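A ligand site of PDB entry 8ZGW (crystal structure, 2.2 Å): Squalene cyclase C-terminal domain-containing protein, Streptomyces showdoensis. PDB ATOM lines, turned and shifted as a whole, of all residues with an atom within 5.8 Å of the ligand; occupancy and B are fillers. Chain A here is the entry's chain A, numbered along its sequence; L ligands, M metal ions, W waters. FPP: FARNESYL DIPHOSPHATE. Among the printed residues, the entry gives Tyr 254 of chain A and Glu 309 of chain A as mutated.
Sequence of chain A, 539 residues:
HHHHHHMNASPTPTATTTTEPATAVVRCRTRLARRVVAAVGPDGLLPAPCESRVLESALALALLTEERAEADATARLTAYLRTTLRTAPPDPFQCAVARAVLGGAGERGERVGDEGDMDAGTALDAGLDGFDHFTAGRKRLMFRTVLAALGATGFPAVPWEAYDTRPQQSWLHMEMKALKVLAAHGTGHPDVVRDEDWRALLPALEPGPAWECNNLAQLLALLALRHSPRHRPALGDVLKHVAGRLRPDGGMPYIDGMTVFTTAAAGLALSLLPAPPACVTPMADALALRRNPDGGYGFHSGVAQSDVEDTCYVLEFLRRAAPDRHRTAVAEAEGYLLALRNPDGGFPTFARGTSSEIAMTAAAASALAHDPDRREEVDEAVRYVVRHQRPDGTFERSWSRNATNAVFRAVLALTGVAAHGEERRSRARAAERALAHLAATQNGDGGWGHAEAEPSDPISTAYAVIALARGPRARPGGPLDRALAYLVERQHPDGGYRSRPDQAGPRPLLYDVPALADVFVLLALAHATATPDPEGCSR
The side-chain amide oxygen (OE1) of Gln 169 sits close to an oxygen (O2A) of the ligand, 2.4 Å away.
An oxygen (O2A) of the ligand sits at hydrogen-bond distance from the indole nitrogen (NE1) of Trp 171 (2.7 Å).
The backbone NH (N) of Arg 507 is in hydrogen-bond range of an oxygen (O1B) of the ligand, at 3.0 Å.
The guanidinium group of Arg 507 is in salt-bridge range of an oxygen (O3B) of the ligand (2.8 Å).
NZ of Lys 139 lies within salt-bridge range of O2B of the ligand, at 2.8 Å.
An oxygen (O1) of the ligand is in hydrogen-bond range of the side-chain hydroxyl (OH) of Tyr 254, 2.9 Å away.
NH2 of Arg 138 lies within salt-bridge range of O2B of the ligand, 3.0 Å away.
The backbone carbonyl oxygen (O) of Gln 503 is in hydrogen-bond range of the backbone NH (N) of Tyr 511, 3.0 Å away.
SD of Met 258 sits at hydrogen-bond distance from OH of Tyr 511 (3.4 Å).
The indole nitrogen (NE1) of Trp 399 sits at hydrogen-bond distance from the side-chain hydroxyl (OG1) of Thr 349 (2.9 Å).
The backbone carbonyl oxygen of Trp 399 lies within hydrogen-bond range of the backbone NH of Ala 504.
The backbone NH (N) of Asp 310 lies within hydrogen-bond range of the side-chain carboxylate (OD1) of Asp 307 (2.7 Å).
N of Phe 261 lies close to OD1 of Asp 310.
The side-chain carboxylate of Asp 307 is in hydrogen-bond range of the backbone NH of Glu 309, 3.0 Å away.
The backbone NH (N) of Phe 261 lies within hydrogen-bond range of the backbone carbonyl oxygen (O) of Phe 299, at 3.2 Å.
Ile 255 touches the ligand.
Met 258 touches the ligand (CE to C14, 3.7 Å).
Phe 261 touches the ligand.
CE1 of Phe 299 touches C4 of the ligand (3.7 Å).
OD2 of Asp 307 touches C10 of the ligand, at 3.3 Å.
OE2 of Glu 309 touches C15 of the ligand, 3.6 Å away.
Asp 310 touches the ligand.
Phe 350 touches the ligand.
Trp 399 touches the ligand (CH2 to O3A, 3.1 Å).
Gln 503 touches the ligand (OE1 to C15, 3.0 Å).
CA of Gly 505 touches O1 of the ligand, 3.9 Å away.
CA of Pro 506 touches O1A of the ligand, 3.5 Å away.
Tyr 511 touches the ligand.
Hydrophobic or aromatic side chains that line the ligand: Trp 171, Ile 255, Met 258, Phe 261, Phe 299, Phe 350, Trp 399, Pro 506 and Tyr 511.
Within 4 Å of the ligand: Arg 138, Lys 139, Gln 169, Trp 171, Tyr 254, Ile 255, Met 258, Phe 261, Phe 299, Asp 307, Glu 309, Asp 310, Phe 350, Trp 399, Gln 503, Gly 505, Pro 506, Arg 507 and Tyr 511.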
ATOM      1  N   THR A 135     -21.764 -30.498 -12.805  1.00  0.00           N
ATOM      2  CA  THR A 135     -22.165 -30.327 -11.376  1.00  0.00           C
ATOM      3  C   THR A 135     -23.624 -29.875 -11.255  1.00  0.00           C
ATOM      4  O   THR A 135     -24.192 -30.065 -10.175  1.00  0.00           O
ATOM      5  CB  THR A 135     -21.263 -29.303 -10.677  1.00  0.00           C
ATOM      6  OG1 THR A 135     -21.459 -29.436  -9.271  1.00  0.00           O
ATOM      7  CG2 THR A 135     -21.548 -27.885 -11.101  1.00  0.00           C
ATOM      8  N   ARG A 138     -26.862 -31.153  -8.748  1.00  0.00           N
ATOM      9  CA  ARG A 138     -26.409 -31.142  -7.339  1.00  0.00           C
ATOM     10  C   ARG A 138     -26.484 -29.689  -6.868  1.00  0.00           C
ATOM     11  O   ARG A 138     -26.943 -29.457  -5.743  1.00  0.00           O
ATOM     12  CB  ARG A 138     -24.979 -31.692  -7.238  1.00  0.00           C
ATOM     13  CG  ARG A 138     -24.213 -31.202  -6.016  1.00  0.00           C
ATOM     14  CD  ARG A 138     -22.993 -32.058  -5.741  1.00  0.00           C
ATOM     15  NE  ARG A 138     -21.781 -31.552  -6.374  1.00  0.00           N
ATOM     16  CZ  ARG A 138     -21.171 -30.430  -6.023  1.00  0.00           C
ATOM     17  NH1 ARG A 138     -21.679 -29.690  -5.044  1.00  0.00           N
ATOM     18  NH2 ARG A 138     -20.071 -30.042  -6.637  1.00  0.00           N
ATOM     19  N   LYS A 139     -26.061 -28.753  -7.716  1.00  0.00           N
ATOM     20  CA  LYS A 139     -26.073 -27.305  -7.350  1.00  0.00           C
ATOM     21  C   LYS A 139     -27.519 -26.817  -7.256  1.00  0.00           C
ATOM     22  O   LYS A 139     -27.792 -26.049  -6.340  1.00  0.00           O
ATOM     23  CB  LYS A 139     -25.228 -26.493  -8.321  1.00  0.00           C
ATOM     24  CG  LYS A 139     -23.912 -27.126  -8.727  1.00  0.00           C
ATOM     25  CD  LYS A 139     -22.756 -26.162  -8.703  1.00  0.00           C
ATOM     26  CE  LYS A 139     -21.515 -26.703  -8.029  1.00  0.00           C
ATOM     27  NZ  LYS A 139     -21.732 -26.911  -6.583  1.00  0.00           N
ATOM     28  N   MET A 142     -28.497 -28.065  -3.838  1.00  0.00           N
ATOM     29  CA  MET A 142     -27.778 -27.306  -2.820  1.00  0.00           C
ATOM     30  C   MET A 142     -28.355 -25.905  -2.660  1.00  0.00           C
ATOM     31  O   MET A 142     -28.711 -25.501  -1.547  1.00  0.00           O
ATOM     32  CB  MET A 142     -26.295 -27.272  -3.206  1.00  0.00           C
ATOM     33  CG  MET A 142     -25.444 -26.169  -2.551  1.00  0.00           C
ATOM     34  SD  MET A 142     -23.704 -26.352  -3.022  1.00  0.00           S
ATOM     35  CE  MET A 142     -23.604 -28.121  -3.260  1.00  0.00           C
ATOM     36  N   GLN A 169     -13.961 -33.896  -3.010  1.00  0.00           N
ATOM     37  CA  GLN A 169     -13.638 -32.710  -2.215  1.00  0.00           C
ATOM     38  C   GLN A 169     -14.029 -32.922  -0.756  1.00  0.00           C
ATOM     39  O   GLN A 169     -15.196 -33.167  -0.449  1.00  0.00           O
ATOM     40  CB  GLN A 169     -14.410 -31.503  -2.784  1.00  0.00           C
ATOM     41  CG  GLN A 169     -14.851 -31.698  -4.229  1.00  0.00           C
ATOM     42  CD  GLN A 169     -15.729 -30.580  -4.729  1.00  0.00           C
ATOM     43  OE1 GLN A 169     -15.384 -29.410  -4.600  1.00  0.00           O
ATOM     44  NE2 GLN A 169     -16.856 -30.927  -5.347  1.00  0.00           N
ATOM     45  N   TRP A 171     -14.703 -31.089   1.720  1.00  0.00           N
ATOM     46  CA  TRP A 171     -15.752 -30.229   2.246  1.00  0.00           C
ATOM     47  C   TRP A 171     -17.063 -30.314   1.463  1.00  0.00           C
ATOM     48  O   TRP A 171     -18.083 -29.788   1.943  1.00  0.00           O
ATOM     49  CB  TRP A 171     -15.281 -28.768   2.255  1.00  0.00           C
ATOM     50  CG  TRP A 171     -14.766 -28.321   0.904  1.00  0.00           C
ATOM     51  CD1 TRP A 171     -15.503 -27.813  -0.126  1.00  0.00           C
ATOM     52  CD2 TRP A 171     -13.402 -28.343   0.434  1.00  0.00           C
ATOM     53  NE1 TRP A 171     -14.698 -27.507  -1.201  1.00  0.00           N
ATOM     54  CE2 TRP A 171     -13.396 -27.828  -0.883  1.00  0.00           C
ATOM     55  CE3 TRP A 171     -12.186 -28.734   1.008  1.00  0.00           C
ATOM     56  CZ2 TRP A 171     -12.228 -27.694  -1.640  1.00  0.00           C
ATOM     57  CZ3 TRP A 171     -11.027 -28.603   0.256  1.00  0.00           C
ATOM     58  CH2 TRP A 171     -11.061 -28.091  -1.052  1.00  0.00           C
ATOM     59  N   LEU A 172     -17.089 -30.925   0.284  1.00  0.00           N
ATOM     60  CA  LEU A 172     -18.375 -31.088  -0.387  1.00  0.00           C
ATOM     61  C   LEU A 172     -19.279 -32.041   0.396  1.00  0.00           C
ATOM     62  O   LEU A 172     -20.492 -31.817   0.497  1.00  0.00           O
ATOM     63  CB  LEU A 172     -18.171 -31.582  -1.810  1.00  0.00           C
ATOM     64  CG  LEU A 172     -19.500 -31.745  -2.570  1.00  0.00           C
ATOM     65  CD1 LEU A 172     -20.291 -30.422  -2.562  1.00  0.00           C
ATOM     66  CD2 LEU A 172     -19.255 -32.246  -3.982  1.00  0.00           C
ATOM     67  N   GLU A 175     -20.771 -30.175   3.327  1.00  0.00           N
ATOM     68  CA  GLU A 175     -21.804 -29.242   2.890  1.00  0.00           C
ATOM     69  C   GLU A 175     -23.115 -29.956   2.591  1.00  0.00           C
ATOM     70  O   GLU A 175     -24.199 -29.523   3.011  1.00  0.00           O
ATOM     71  CB  GLU A 175     -21.316 -28.463   1.659  1.00  0.00           C
ATOM     72  CG  GLU A 175     -20.456 -27.243   1.986  1.00  0.00           C
ATOM     73  CD  GLU A 175     -19.619 -26.770   0.799  1.00  0.00           C
ATOM     74  OE1 GLU A 175     -19.763 -27.321  -0.318  1.00  0.00           O
ATOM     75  OE2 GLU A 175     -18.812 -25.824   0.982  1.00  0.00           O
ATOM     76  N   ASN A 214     -12.581 -23.230   4.896  1.00  0.00           N
ATOM     77  CA  ASN A 214     -13.850 -23.013   4.177  1.00  0.00           C
ATOM     78  C   ASN A 214     -14.913 -22.532   5.154  1.00  0.00           C
ATOM     79  O   ASN A 214     -15.532 -23.324   5.874  1.00  0.00           O
ATOM     80  CB  ASN A 214     -14.283 -24.293   3.462  1.00  0.00           C
ATOM     81  CG  ASN A 214     -15.360 -24.055   2.424  1.00  0.00           C
ATOM     82  OD1 ASN A 214     -16.342 -23.347   2.668  1.00  0.00           O
ATOM     83  ND2 ASN A 214     -15.176 -24.646   1.243  1.00  0.00           N
ATOM     84  N   TYR A 254     -15.412 -15.957   1.969  1.00  0.00           N
ATOM     85  CA  TYR A 254     -15.690 -17.351   1.638  1.00  0.00           C
ATOM     86  C   TYR A 254     -14.652 -18.273   2.255  1.00  0.00           C
ATOM     87  O   TYR A 254     -14.986 -19.252   2.939  1.00  0.00           O
ATOM     88  CB  TYR A 254     -15.744 -17.505   0.122  1.00  0.00           C
ATOM     89  CG  TYR A 254     -15.768 -18.921  -0.397  1.00  0.00           C
ATOM     90  CD1 TYR A 254     -16.519 -19.914   0.237  1.00  0.00           C
ATOM     91  CD2 TYR A 254     -15.077 -19.261  -1.538  1.00  0.00           C
ATOM     92  CE1 TYR A 254     -16.557 -21.201  -0.273  1.00  0.00           C
ATOM     93  CE2 TYR A 254     -15.105 -20.519  -2.039  1.00  0.00           C
ATOM     94  CZ  TYR A 254     -15.844 -21.495  -1.417  1.00  0.00           C
ATOM     95  OH  TYR A 254     -15.838 -22.762  -1.968  1.00  0.00           O
ATOM     96  N   ILE A 255     -13.366 -17.979   2.028  1.00  0.00           N
ATOM     97  CA  ILE A 255     -12.247 -18.800   2.483  1.00  0.00           C
ATOM     98  C   ILE A 255     -11.243 -17.868   3.164  1.00  0.00           C
ATOM     99  O   ILE A 255     -11.309 -16.651   3.028  1.00  0.00           O
ATOM    100  CB  ILE A 255     -11.589 -19.560   1.315  1.00  0.00           C
ATOM    101  CG1 ILE A 255     -11.205 -18.579   0.197  1.00  0.00           C
ATOM    102  CG2 ILE A 255     -12.558 -20.595   0.753  1.00  0.00           C
ATOM    103  CD1 ILE A 255     -10.724 -19.256  -1.090  1.00  0.00           C
ATOM    104  N   MET A 258      -5.891 -17.655  -0.480  1.00  0.00           N
ATOM    105  CA  MET A 258      -5.417 -18.549  -1.529  1.00  0.00           C
ATOM    106  C   MET A 258      -3.910 -18.401  -1.694  1.00  0.00           C
ATOM    107  O   MET A 258      -3.388 -18.337  -2.811  1.00  0.00           O
ATOM    108  CB  MET A 258      -6.122 -18.264  -2.854  1.00  0.00           C
ATOM    109  CG  MET A 258      -7.282 -19.193  -3.175  1.00  0.00           C
ATOM    110  SD  MET A 258      -8.048 -18.690  -4.735  1.00  0.00           S
ATOM    111  CE  MET A 258      -7.487 -20.076  -5.740  1.00  0.00           C
ATOM    112  N   PHE A 261      -1.885 -21.167  -4.013  1.00  0.00           N
ATOM    113  CA  PHE A 261      -2.181 -20.896  -5.412  1.00  0.00           C
ATOM    114  C   PHE A 261      -1.528 -19.605  -5.901  1.00  0.00           C
ATOM    115  O   PHE A 261      -0.856 -19.583  -6.938  1.00  0.00           O
ATOM    116  CB  PHE A 261      -3.703 -20.827  -5.598  1.00  0.00           C
ATOM    117  CG  PHE A 261      -4.146 -20.563  -7.001  1.00  0.00           C
ATOM    118  CD1 PHE A 261      -3.943 -21.501  -7.999  1.00  0.00           C
ATOM    119  CD2 PHE A 261      -4.787 -19.377  -7.330  1.00  0.00           C
ATOM    120  CE1 PHE A 261      -4.344 -21.264  -9.303  1.00  0.00           C
ATOM    121  CE2 PHE A 261      -5.214 -19.127  -8.636  1.00  0.00           C
ATOM    122  CZ  PHE A 261      -4.988 -20.075  -9.615  1.00  0.00           C
ATOM    123  N   PHE A 299      -4.979 -25.008  -1.787  1.00  0.00           N
ATOM    124  CA  PHE A 299      -4.975 -23.625  -2.262  1.00  0.00           C
ATOM    125  C   PHE A 299      -4.438 -22.616  -1.226  1.00  0.00           C
ATOM    126  O   PHE A 299      -3.989 -21.544  -1.628  1.00  0.00           O
ATOM    127  CB  PHE A 299      -6.388 -23.202  -2.716  1.00  0.00           C
ATOM    128  CG  PHE A 299      -7.457 -23.311  -1.626  1.00  0.00           C
ATOM    129  CD1 PHE A 299      -8.159 -24.494  -1.446  1.00  0.00           C
ATOM    130  CD2 PHE A 299      -7.769 -22.217  -0.827  1.00  0.00           C
ATOM    131  CE1 PHE A 299      -9.150 -24.601  -0.452  1.00  0.00           C
ATOM    132  CE2 PHE A 299      -8.742 -22.321   0.158  1.00  0.00           C
ATOM    133  CZ  PHE A 299      -9.426 -23.510   0.350  1.00  0.00           C
ATOM    134  N   ASP A 307      -5.360 -30.593  -4.809  1.00  0.00           N
ATOM    135  CA  ASP A 307      -6.077 -30.500  -6.084  1.00  0.00           C
ATOM    136  C   ASP A 307      -5.100 -30.333  -7.242  1.00  0.00           C
ATOM    137  O   ASP A 307      -3.963 -29.886  -7.075  1.00  0.00           O
ATOM    138  CB  ASP A 307      -7.097 -29.355  -6.068  1.00  0.00           C
ATOM    139  CG  ASP A 307      -6.430 -27.982  -6.068  1.00  0.00           C
ATOM    140  OD1 ASP A 307      -6.090 -27.468  -7.166  1.00  0.00           O
ATOM    141  OD2 ASP A 307      -6.236 -27.425  -4.965  1.00  0.00           O
ATOM    142  N   GLU A 309      -5.151 -28.335  -9.912  1.00  0.00           N
ATOM    143  CA  GLU A 309      -4.797 -26.983 -10.357  1.00  0.00           C
ATOM    144  C   GLU A 309      -3.658 -26.401  -9.514  1.00  0.00           C
ATOM    145  O   GLU A 309      -2.672 -25.857 -10.058  1.00  0.00           O
ATOM    146  CB  GLU A 309      -6.008 -26.057 -10.299  1.00  0.00           C
ATOM    147  CG  GLU A 309      -5.670 -24.593 -10.563  1.00  0.00           C
ATOM    148  CD  GLU A 309      -6.246 -24.094 -11.897  1.00  0.00           C
ATOM    149  OE1 GLU A 309      -5.542 -24.226 -12.916  1.00  0.00           O
ATOM    150  OE2 GLU A 309      -7.387 -23.580 -11.909  1.00  0.00           O
ATOM    151  N   ASP A 310      -3.780 -26.484  -8.189  1.00  0.00           N
ATOM    152  CA  ASP A 310      -2.704 -25.978  -7.347  1.00  0.00           C
ATOM    153  C   ASP A 310      -1.414 -26.738  -7.586  1.00  0.00           C
ATOM    154  O   ASP A 310      -0.342 -26.134  -7.668  1.00  0.00           O
ATOM    155  CB  ASP A 310      -3.091 -26.048  -5.884  1.00  0.00           C
ATOM    156  CG  ASP A 310      -4.037 -24.968  -5.512  1.00  0.00           C
ATOM    157  OD1 ASP A 310      -3.547 -23.827  -5.308  1.00  0.00           O
ATOM    158  OD2 ASP A 310      -5.259 -25.230  -5.397  1.00  0.00           O
ATOM    159  N   THR A 349     -10.335 -32.732 -10.879  1.00  0.00           N
ATOM    160  CA  THR A 349      -9.804 -31.680 -10.021  1.00  0.00           C
ATOM    161  C   THR A 349      -9.238 -32.244  -8.714  1.00  0.00           C
ATOM    162  O   THR A 349      -8.147 -31.845  -8.290  1.00  0.00           O
ATOM    163  CB  THR A 349     -10.895 -30.664  -9.697  1.00  0.00           C
ATOM    164  OG1 THR A 349     -11.413 -30.113 -10.911  1.00  0.00           O
ATOM    165  CG2 THR A 349     -10.337 -29.534  -8.840  1.00  0.00           C
ATOM    166  N   PHE A 350      -9.971 -33.152  -8.073  1.00  0.00           N
ATOM    167  CA  PHE A 350      -9.720 -33.586  -6.703  1.00  0.00           C
ATOM    168  C   PHE A 350      -9.516 -35.089  -6.579  1.00  0.00           C
ATOM    169  O   PHE A 350      -8.735 -35.530  -5.731  1.00  0.00           O
ATOM    170  CB  PHE A 350     -10.910 -33.228  -5.788  1.00  0.00           C
ATOM    171  CG  PHE A 350     -11.220 -31.761  -5.679  1.00  0.00           C
ATOM    172  CD1 PHE A 350     -10.359 -30.895  -4.996  1.00  0.00           C
ATOM    173  CD2 PHE A 350     -12.389 -31.245  -6.193  1.00  0.00           C
ATOM    174  CE1 PHE A 350     -10.676 -29.540  -4.862  1.00  0.00           C
ATOM    175  CE2 PHE A 350     -12.690 -29.895  -6.071  1.00  0.00           C
ATOM    176  CZ  PHE A 350     -11.837 -29.058  -5.398  1.00  0.00           C
ATOM    177  N   MET A 360      -8.242 -28.896 -16.276  1.00  0.00           N
ATOM    178  CA  MET A 360      -7.416 -29.731 -15.400  1.00  0.00           C
ATOM    179  C   MET A 360      -6.518 -30.655 -16.221  1.00  0.00           C
ATOM    180  O   MET A 360      -5.363 -30.902 -15.868  1.00  0.00           O
ATOM    181  CB  MET A 360      -8.297 -30.567 -14.470  1.00  0.00           C
ATOM    182  CG  MET A 360      -9.098 -29.798 -13.428  1.00  0.00           C
ATOM    183  SD  MET A 360      -8.146 -28.663 -12.411  1.00  0.00           S
ATOM    184  CE  MET A 360      -8.184 -27.174 -13.416  1.00  0.00           C
ATOM    185  N   TRP A 399     -13.630 -23.710 -13.018  1.00  0.00           N
ATOM    186  CA  TRP A 399     -13.153 -22.975 -11.856  1.00  0.00           C
ATOM    187  C   TRP A 399     -12.960 -21.484 -12.148  1.00  0.00           C
ATOM    188  O   TRP A 399     -12.766 -20.706 -11.201  1.00  0.00           O
ATOM    189  CB  TRP A 399     -11.850 -23.601 -11.350  1.00  0.00           C
ATOM    190  CG  TRP A 399     -12.040 -25.014 -10.830  1.00  0.00           C
ATOM    191  CD1 TRP A 399     -11.391 -26.124 -11.267  1.00  0.00           C
ATOM    192  CD2 TRP A 399     -12.918 -25.444  -9.774  1.00  0.00           C
ATOM    193  NE1 TRP A 399     -11.796 -27.229 -10.553  1.00  0.00           N
ATOM    194  CE2 TRP A 399     -12.740 -26.844  -9.632  1.00  0.00           C
ATOM    195  CE3 TRP A 399     -13.837 -24.786  -8.933  1.00  0.00           C
ATOM    196  CZ2 TRP A 399     -13.454 -27.606  -8.676  1.00  0.00           C
ATOM    197  CZ3 TRP A 399     -14.543 -25.556  -7.985  1.00  0.00           C
ATOM    198  CH2 TRP A 399     -14.334 -26.943  -7.869  1.00  0.00           C
ATOM    199  N   GLN A 503     -12.596 -16.083 -10.020  1.00  0.00           N
ATOM    200  CA  GLN A 503     -12.630 -17.370  -9.353  1.00  0.00           C
ATOM    201  C   GLN A 503     -14.053 -17.674  -8.898  1.00  0.00           C
ATOM    202  O   GLN A 503     -14.782 -16.792  -8.426  1.00  0.00           O
ATOM    203  CB  GLN A 503     -11.682 -17.395  -8.156  1.00  0.00           C
ATOM    204  CG  GLN A 503     -10.194 -17.237  -8.520  1.00  0.00           C
ATOM    205  CD  GLN A 503      -9.717 -18.300  -9.478  1.00  0.00           C
ATOM    206  OE1 GLN A 503     -10.012 -19.495  -9.306  1.00  0.00           O
ATOM    207  NE2 GLN A 503      -8.992 -17.883 -10.525  1.00  0.00           N
ATOM    208  N   ALA A 504     -14.447 -18.930  -9.052  1.00  0.00           N
ATOM    209  CA  ALA A 504     -15.765 -19.393  -8.663  1.00  0.00           C
ATOM    210  C   ALA A 504     -15.646 -20.536  -7.660  1.00  0.00           C
ATOM    211  O   ALA A 504     -14.722 -21.347  -7.718  1.00  0.00           O
ATOM    212  CB  ALA A 504     -16.575 -19.828  -9.882  1.00  0.00           C
ATOM    213  N   GLY A 505     -16.603 -20.589  -6.735  1.00  0.00           N
ATOM    214  CA  GLY A 505     -16.646 -21.610  -5.726  1.00  0.00           C
ATOM    215  C   GLY A 505     -17.624 -21.244  -4.629  1.00  0.00           C
ATOM    216  O   GLY A 505     -17.558 -20.155  -4.058  1.00  0.00           O
ATOM    217  N   PRO A 506     -18.620 -22.114  -4.396  1.00  0.00           N
ATOM    218  CA  PRO A 506     -19.057 -23.225  -5.251  1.00  0.00           C
ATOM    219  C   PRO A 506     -19.424 -22.686  -6.625  1.00  0.00           C
ATOM    220  O   PRO A 506     -20.098 -21.658  -6.722  1.00  0.00           O
ATOM    221  CB  PRO A 506     -20.329 -23.756  -4.543  1.00  0.00           C
ATOM    222  CG  PRO A 506     -20.271 -23.211  -3.163  1.00  0.00           C
ATOM    223  CD  PRO A 506     -19.535 -21.902  -3.261  1.00  0.00           C
ATOM    224  N   ARG A 507     -19.030 -23.359  -7.693  1.00  0.00           N
ATOM    225  CA  ARG A 507     -19.374 -22.895  -9.030  1.00  0.00           C
ATOM    226  C   ARG A 507     -20.893 -22.709  -9.134  1.00  0.00           C
ATOM    227  O   ARG A 507     -21.644 -23.546  -8.637  1.00  0.00           O
ATOM    228  CB  ARG A 507     -18.868 -23.888 -10.084  1.00  0.00           C
ATOM    229  CG  ARG A 507     -17.338 -23.813 -10.236  1.00  0.00           C
ATOM    230  CD  ARG A 507     -16.755 -25.020 -10.949  1.00  0.00           C
ATOM    231  NE  ARG A 507     -16.885 -26.240 -10.166  1.00  0.00           N
ATOM    232  CZ  ARG A 507     -16.258 -27.380 -10.453  1.00  0.00           C
ATOM    233  NH1 ARG A 507     -15.448 -27.489 -11.498  1.00  0.00           N
ATOM    234  NH2 ARG A 507     -16.454 -28.436  -9.661  1.00  0.00           N
ATOM    235  N   TYR A 511     -15.979 -15.416  -6.095  1.00  0.00           N
ATOM    236  CA  TYR A 511     -15.394 -14.824  -4.916  1.00  0.00           C
ATOM    237  C   TYR A 511     -14.140 -14.062  -5.345  1.00  0.00           C
ATOM    238  O   TYR A 511     -13.618 -14.264  -6.443  1.00  0.00           O
ATOM    239  CB  TYR A 511     -15.086 -15.877  -3.854  1.00  0.00           C
ATOM    240  CG  TYR A 511     -14.074 -16.900  -4.274  1.00  0.00           C
ATOM    241  CD1 TYR A 511     -14.464 -18.070  -4.920  1.00  0.00           C
ATOM    242  CD2 TYR A 511     -12.724 -16.710  -4.020  1.00  0.00           C
ATOM    243  CE1 TYR A 511     -13.545 -19.008  -5.305  1.00  0.00           C
ATOM    244  CE2 TYR A 511     -11.787 -17.646  -4.390  1.00  0.00           C
ATOM    245  CZ  TYR A 511     -12.199 -18.798  -5.026  1.00  0.00           C
ATOM    246  OH  TYR A 511     -11.257 -19.728  -5.383  1.00  0.00           O
HETATM  247  C1  FPP L   1     -14.185 -24.997  -4.178  1.00  0.00           C
HETATM  248  O1  FPP L   1     -15.566 -24.866  -3.973  1.00  0.00           O
HETATM  249  C2  FPP L   1     -13.575 -23.587  -4.138  1.00  0.00           C
HETATM  250  C3  FPP L   1     -12.302 -23.508  -3.298  1.00  0.00           C
HETATM  251  C4  FPP L   1     -12.477 -23.660  -1.786  1.00  0.00           C
HETATM  252  C5  FPP L   1     -11.406 -22.335  -3.712  1.00  0.00           C
HETATM  253  C6  FPP L   1     -10.843 -22.639  -5.102  1.00  0.00           C
HETATM  254  C7  FPP L   1      -9.761 -23.709  -4.978  1.00  0.00           C
HETATM  255  C8  FPP L   1     -10.243 -25.100  -5.376  1.00  0.00           C
HETATM  256  C10 FPP L   1      -9.360 -26.241  -4.853  1.00  0.00           C
HETATM  257  C9  FPP L   1     -10.640 -25.193  -6.848  1.00  0.00           C
HETATM  258  C11 FPP L   1      -9.430 -25.586  -7.716  1.00  0.00           C
HETATM  259  C12 FPP L   1      -9.092 -24.433  -8.683  1.00  0.00           C
HETATM  260  C13 FPP L   1      -8.507 -23.203  -7.983  1.00  0.00           C
HETATM  261  C14 FPP L   1      -7.222 -23.498  -7.198  1.00  0.00           C
HETATM  262  C15 FPP L   1      -8.403 -21.969  -8.883  1.00  0.00           C
HETATM  263  PA  FPP L   1     -16.517 -26.177  -4.203  1.00  0.00           P
HETATM  264  O1A FPP L   1     -17.823 -26.013  -3.570  1.00  0.00           O
HETATM  265  O2A FPP L   1     -16.014 -27.356  -3.523  1.00  0.00           O
HETATM  266  O3A FPP L   1     -16.618 -26.428  -5.816  1.00  0.00           O
HETATM  267  PB  FPP L   1     -17.902 -27.121  -6.565  1.00  0.00           P
HETATM  268  O1B FPP L   1     -18.332 -26.260  -7.664  1.00  0.00           O
HETATM  269  O2B FPP L   1     -19.109 -27.360  -5.774  1.00  0.00           O
HETATM  270  O3B FPP L   1     -17.543 -28.440  -7.112  1.00  0.00           O
HETATM  271 MG    MG M   1     -20.191 -27.554  -3.134  1.00  0.00          MG
HETATM  272 MG    MG M   2     -17.511 -24.926  -0.877  1.00  0.00          MG
HETATM  273  O   HOH W   1      -7.297 -27.651  -2.531  1.00  0.00           O
HETATM  274  O   HOH W   2     -11.854 -21.285  -8.155  1.00  0.00           O
